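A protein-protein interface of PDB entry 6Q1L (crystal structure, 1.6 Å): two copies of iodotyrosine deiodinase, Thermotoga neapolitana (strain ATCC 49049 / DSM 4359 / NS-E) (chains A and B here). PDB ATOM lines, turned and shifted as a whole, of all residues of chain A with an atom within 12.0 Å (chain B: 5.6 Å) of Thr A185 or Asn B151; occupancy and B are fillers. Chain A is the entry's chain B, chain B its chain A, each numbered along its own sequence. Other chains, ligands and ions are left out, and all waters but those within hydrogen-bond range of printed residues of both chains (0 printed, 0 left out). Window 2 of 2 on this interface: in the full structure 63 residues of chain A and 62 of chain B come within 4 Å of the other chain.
O of Val B150 is in hydrogen-bond range of N of Phe A186, at 3.0 Å.
OG1 of Thr B152 lies within hydrogen-bond range of O of Glu B147 (2.8 Å).
CA of Leu B49 touches O of Arg A182 (3.5 Å). C of Tyr A183 touches CD1 of Leu B49 (3.8 Å). Leu B56 touches Asn A184 (CD2 to O, 3.1 Å). Val B150 touches Asn A184. Leu B49 touches Thr A185. Thr A185 touches Leu B56. CA of Thr A185 touches O of Val B150, 3.6 Å away. ND2 of Asn B151 touches CB of Thr A185, at 3.8 Å. CA of Thr B152 touches CD1 of Phe A186 (3.8 Å). Pro B153 touches Phe A186 (CD to CG, 3.6 Å).
Of the printed residues of chain B, Thr A185 touches Leu B49 (3.8 Å), Leu B56 (3.7 Å), Val B150 (3.6 Å) and Asn B151 (3.8 Å). Printed residues of chain A within 4 Å of Asn B151: Thr A185 and Phe A186. Pro B153 touches just one residue of chain A: Phe A186. Of the printed residues of chain B, Arg A182 touches Leu B49 (3.5 Å). Of the printed residues of chain B, Tyr A183 touches Leu B49 (3.8 Å). Of the printed residues of chain B, Phe A186 touches Val B150 (3.0 Å), Asn B151 (3.2 Å), Thr B152 (3.8 Å) and Pro B153 (3.6 Å). Of the printed residues of chain B, Asn A184 touches Leu B49 (3.4 Å), Leu B56 (3.1 Å) and Val B150 (3.4 Å). Val B146 touches none of the printed residues of chain A. The nearest printed residue of chain A that does not touch Asn B151 is Asn A184 (6.5 Å). The nearest printed residue of chain B that does not touch Arg A182 is Pro B153 (6.2 Å).
Printed residues of chain A that touch a printed residue of chain B: Arg A182, Tyr A183, Asn A184, Thr A185 and Phe A186. Hydrophobic or aromatic side chains of chain A within 4 Å of the printed part of chain B: Phe A186. Among the printed residues, 13 pairs touch across the chains. Among the printed residues, no Asp or Glu carboxylate lies within 4 Å of a Lys or Arg side-chain nitrogen of the other chain.
No position is printed for both chains.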
ATOM      1  N   ILE A 180      -0.274  14.999  42.849  1.00  0.00           N
ATOM      2  CA  ILE A 180       0.138  13.850  42.055  1.00  0.00           C
ATOM      3  C   ILE A 180       0.374  14.358  40.640  1.00  0.00           C
ATOM      4  O   ILE A 180      -0.567  14.742  39.930  1.00  0.00           O
ATOM      5  CB  ILE A 180      -0.881  12.708  42.069  1.00  0.00           C
ATOM      6  CG1 ILE A 180      -1.117  12.225  43.502  1.00  0.00           C
ATOM      7  CG2 ILE A 180      -0.345  11.561  41.213  1.00  0.00           C
ATOM      8  CD1 ILE A 180      -2.257  11.274  43.618  1.00  0.00           C
ATOM      9  N   VAL A 181       1.607  14.361  40.243  1.00  0.00           N
ATOM     10  CA  VAL A 181       1.974  14.851  38.933  1.00  0.00           C
ATOM     11  C   VAL A 181       1.893  13.693  37.956  1.00  0.00           C
ATOM     12  O   VAL A 181       1.909  12.513  38.325  1.00  0.00           O
ATOM     13  CB  VAL A 181       3.371  15.475  38.934  1.00  0.00           C
ATOM     14  CG1 VAL A 181       3.471  16.498  40.033  1.00  0.00           C
ATOM     15  CG2 VAL A 181       4.453  14.410  39.059  1.00  0.00           C
ATOM     16  N   ARG A 182       1.756  14.050  36.702  1.00  0.00           N
ATOM     17  CA  ARG A 182       1.976  13.167  35.582  1.00  0.00           C
ATOM     18  C   ARG A 182       3.105  13.730  34.741  1.00  0.00           C
ATOM     19  O   ARG A 182       3.469  14.903  34.863  1.00  0.00           O
ATOM     20  CB  ARG A 182       0.698  13.022  34.768  1.00  0.00           C
ATOM     21  CG  ARG A 182      -0.425  12.379  35.541  1.00  0.00           C
ATOM     22  CD  ARG A 182      -1.693  12.491  34.748  1.00  0.00           C
ATOM     23  NE  ARG A 182      -2.751  11.579  35.186  1.00  0.00           N
ATOM     24  CZ  ARG A 182      -3.766  11.925  35.981  1.00  0.00           C
ATOM     25  NH1 ARG A 182      -3.880  13.159  36.460  1.00  0.00           N
ATOM     26  NH2 ARG A 182      -4.684  11.022  36.291  1.00  0.00           N
ATOM     27  N   TYR A 183       3.681  12.863  33.924  1.00  0.00           N
ATOM     28  CA  TYR A 183       4.813  13.197  33.092  1.00  0.00           C
ATOM     29  C   TYR A 183       4.480  12.939  31.640  1.00  0.00           C
ATOM     30  O   TYR A 183       4.003  11.861  31.274  1.00  0.00           O
ATOM     31  CB  TYR A 183       6.071  12.409  33.468  1.00  0.00           C
ATOM     32  CG  TYR A 183       6.524  12.686  34.853  1.00  0.00           C
ATOM     33  CD1 TYR A 183       5.974  12.000  35.919  1.00  0.00           C
ATOM     34  CD2 TYR A 183       7.478  13.652  35.105  1.00  0.00           C
ATOM     35  CE1 TYR A 183       6.366  12.266  37.202  1.00  0.00           C
ATOM     36  CE2 TYR A 183       7.865  13.938  36.376  1.00  0.00           C
ATOM     37  CZ  TYR A 183       7.312  13.229  37.427  1.00  0.00           C
ATOM     38  OH  TYR A 183       7.686  13.488  38.727  1.00  0.00           O
ATOM     39  N   ASN A 184       4.768  13.950  30.828  1.00  0.00           N
ATOM     40  CA  ASN A 184       4.712  13.960  29.378  1.00  0.00           C
ATOM     41  C   ASN A 184       3.319  13.797  28.820  1.00  0.00           C
ATOM     42  O   ASN A 184       2.848  14.702  28.125  1.00  0.00           O
ATOM     43  CB  ASN A 184       5.683  12.922  28.842  1.00  0.00           C
ATOM     44  CG  ASN A 184       7.115  13.335  29.057  1.00  0.00           C
ATOM     45  OD1 ASN A 184       7.499  14.483  28.785  1.00  0.00           O
ATOM     46  ND2 ASN A 184       7.918  12.419  29.574  1.00  0.00           N
ATOM     47  N   THR A 185       2.641  12.682  29.094  1.00  0.00           N
ATOM     48  CA  THR A 185       1.294  12.509  28.589  1.00  0.00           C
ATOM     49  C   THR A 185       0.465  11.774  29.623  1.00  0.00           C
ATOM     50  O   THR A 185       0.999  11.180  30.556  1.00  0.00           O
ATOM     51  CB  THR A 185       1.245  11.734  27.263  1.00  0.00           C
ATOM     52  OG1 THR A 185       1.577  10.361  27.509  1.00  0.00           O
ATOM     53  CG2 THR A 185       2.216  12.328  26.249  1.00  0.00           C
ATOM     54  N   PHE A 186      -0.846  11.875  29.457  1.00  0.00           N
ATOM     55  CA  PHE A 186      -1.804  11.118  30.232  1.00  0.00           C
ATOM     56  C   PHE A 186      -1.792   9.697  29.658  1.00  0.00           C
ATOM     57  O   PHE A 186      -1.797   8.746  30.436  1.00  0.00           O
ATOM     58  CB  PHE A 186      -3.202  11.741  30.165  1.00  0.00           C
ATOM     59  CG  PHE A 186      -3.311  13.065  30.882  1.00  0.00           C
ATOM     60  CD1 PHE A 186      -2.986  14.248  30.235  1.00  0.00           C
ATOM     61  CD2 PHE A 186      -3.734  13.131  32.199  1.00  0.00           C
ATOM     62  CE1 PHE A 186      -3.086  15.468  30.893  1.00  0.00           C
ATOM     63  CE2 PHE A 186      -3.821  14.358  32.861  1.00  0.00           C
ATOM     64  CZ  PHE A 186      -3.506  15.519  32.198  1.00  0.00           C
ATOM     65  N   LEU B  49       0.870  18.365  34.537  1.00  0.00           N
ATOM     66  CA  LEU B  49       1.544  17.483  33.592  1.00  0.00           C
ATOM     67  C   LEU B  49       2.904  18.086  33.298  1.00  0.00           C
ATOM     68  O   LEU B  49       3.000  19.208  32.791  1.00  0.00           O
ATOM     69  CB  LEU B  49       0.733  17.337  32.321  1.00  0.00           C
ATOM     70  CG  LEU B  49       1.365  16.440  31.265  1.00  0.00           C
ATOM     71  CD1 LEU B  49       1.335  14.980  31.758  1.00  0.00           C
ATOM     72  CD2 LEU B  49       0.671  16.563  29.941  1.00  0.00           C
ATOM     73  N   LEU B  56       8.244  15.359  22.289  1.00  0.00           N
ATOM     74  CA  LEU B  56       6.952  15.927  22.644  1.00  0.00           C
ATOM     75  C   LEU B  56       7.033  17.446  22.759  1.00  0.00           C
ATOM     76  O   LEU B  56       6.110  18.156  22.341  1.00  0.00           O
ATOM     77  CB  LEU B  56       6.476  15.302  23.949  1.00  0.00           C
ATOM     78  CG  LEU B  56       5.096  15.743  24.407  1.00  0.00           C
ATOM     79  CD1 LEU B  56       4.091  15.424  23.310  1.00  0.00           C
ATOM     80  CD2 LEU B  56       4.675  15.066  25.696  1.00  0.00           C
ATOM     81  N   VAL B 146      -2.950  21.034  21.509  1.00  0.00           N
ATOM     82  CA  VAL B 146      -1.974  20.687  22.533  1.00  0.00           C
ATOM     83  C   VAL B 146      -2.563  19.641  23.470  1.00  0.00           C
ATOM     84  O   VAL B 146      -1.911  18.649  23.805  1.00  0.00           O
ATOM     85  CB  VAL B 146      -1.530  21.949  23.296  1.00  0.00           C
ATOM     86  CG1 VAL B 146      -0.614  21.602  24.436  1.00  0.00           C
ATOM     87  CG2 VAL B 146      -0.824  22.927  22.343  1.00  0.00           C
ATOM     88  N   GLU B 147      -3.817  19.845  23.874  1.00  0.00           N
ATOM     89  CA  GLU B 147      -4.499  18.860  24.712  1.00  0.00           C
ATOM     90  C   GLU B 147      -4.459  17.479  24.073  1.00  0.00           C
ATOM     91  O   GLU B 147      -4.164  16.482  24.748  1.00  0.00           O
ATOM     92  CB  GLU B 147      -5.938  19.292  24.952  1.00  0.00           C
ATOM     93  CG  GLU B 147      -6.124  20.436  25.941  1.00  0.00           C
ATOM     94  CD  GLU B 147      -7.603  20.742  26.153  1.00  0.00           C
ATOM     95  OE1 GLU B 147      -8.431  20.215  25.383  1.00  0.00           O
ATOM     96  OE2 GLU B 147      -7.948  21.487  27.085  1.00  0.00           O
ATOM     97  N   LYS B 148      -4.699  17.409  22.763  1.00  0.00           N
ATOM     98  CA  LYS B 148      -4.730  16.110  22.110  1.00  0.00           C
ATOM     99  C   LYS B 148      -3.348  15.486  22.092  1.00  0.00           C
ATOM    100  O   LYS B 148      -3.211  14.270  22.224  1.00  0.00           O
ATOM    101  CB  LYS B 148      -5.284  16.224  20.696  1.00  0.00           C
ATOM    102  CG  LYS B 148      -5.495  14.856  20.072  1.00  0.00           C
ATOM    103  CD  LYS B 148      -6.219  14.891  18.737  1.00  0.00           C
ATOM    104  CE  LYS B 148      -6.547  13.470  18.282  1.00  0.00           C
ATOM    105  NZ  LYS B 148      -5.361  12.557  18.372  1.00  0.00           N
ATOM    106  N   LEU B 149      -2.302  16.308  21.940  1.00  0.00           N
ATOM    107  CA  LEU B 149      -0.951  15.775  21.893  1.00  0.00           C
ATOM    108  C   LEU B 149      -0.560  15.043  23.164  1.00  0.00           C
ATOM    109  O   LEU B 149       0.288  14.142  23.121  1.00  0.00           O
ATOM    110  CB  LEU B 149       0.035  16.918  21.675  1.00  0.00           C
ATOM    111  CG  LEU B 149       0.322  17.381  20.258  1.00  0.00           C
ATOM    112  CD1 LEU B 149       1.324  18.528  20.349  1.00  0.00           C
ATOM    113  CD2 LEU B 149       0.879  16.238  19.463  1.00  0.00           C
ATOM    114  N   VAL B 150      -1.118  15.426  24.305  1.00  0.00           N
ATOM    115  CA  VAL B 150      -0.766  14.800  25.567  1.00  0.00           C
ATOM    116  C   VAL B 150      -1.893  13.903  26.083  1.00  0.00           C
ATOM    117  O   VAL B 150      -1.903  13.530  27.253  1.00  0.00           O
ATOM    118  CB  VAL B 150      -0.352  15.850  26.608  1.00  0.00           C
ATOM    119  CG1 VAL B 150       0.888  16.624  26.107  1.00  0.00           C
ATOM    120  CG2 VAL B 150      -1.496  16.818  26.903  1.00  0.00           C
ATOM    121  N   ASN B 151      -2.828  13.545  25.211  1.00  0.00           N
ATOM    122  CA  ASN B 151      -3.896  12.602  25.551  1.00  0.00           C
ATOM    123  C   ASN B 151      -4.727  13.120  26.723  1.00  0.00           C
ATOM    124  O   ASN B 151      -5.087  12.368  27.628  1.00  0.00           O
ATOM    125  CB  ASN B 151      -3.317  11.221  25.860  1.00  0.00           C
ATOM    126  CG  ASN B 151      -2.514  10.656  24.706  1.00  0.00           C
ATOM    127  OD1 ASN B 151      -2.902  10.777  23.549  1.00  0.00           O
ATOM    128  ND2 ASN B 151      -1.381  10.045  25.017  1.00  0.00           N
ATOM    129  N   THR B 152      -5.035  14.409  26.703  1.00  0.00           N
ATOM    130  CA  THR B 152      -5.788  14.993  27.799  1.00  0.00           C
ATOM    131  C   THR B 152      -7.144  14.305  27.920  1.00  0.00           C
ATOM    132  O   THR B 152      -7.855  14.160  26.918  1.00  0.00           O
ATOM    133  CB  THR B 152      -5.988  16.488  27.585  1.00  0.00           C
ATOM    134  OG1 THR B 152      -4.709  17.108  27.421  1.00  0.00           O
ATOM    135  CG2 THR B 152      -6.688  17.116  28.748  1.00  0.00           C
ATOM    136  N   PRO B 153      -7.545  13.895  29.112  1.00  0.00           N
ATOM    137  CA  PRO B 153      -8.898  13.348  29.282  1.00  0.00           C
ATOM    138  C   PRO B 153      -9.941  14.444  29.156  1.00  0.00           C
ATOM    139  O   PRO B 153      -9.662  15.614  29.403  1.00  0.00           O
ATOM    140  CB  PRO B 153      -8.875  12.768  30.696  1.00  0.00           C
ATOM    141  CG  PRO B 153      -7.748  13.352  31.372  1.00  0.00           C
ATOM    142  CD  PRO B 153      -6.746  13.832  30.350  1.00  0.00           C
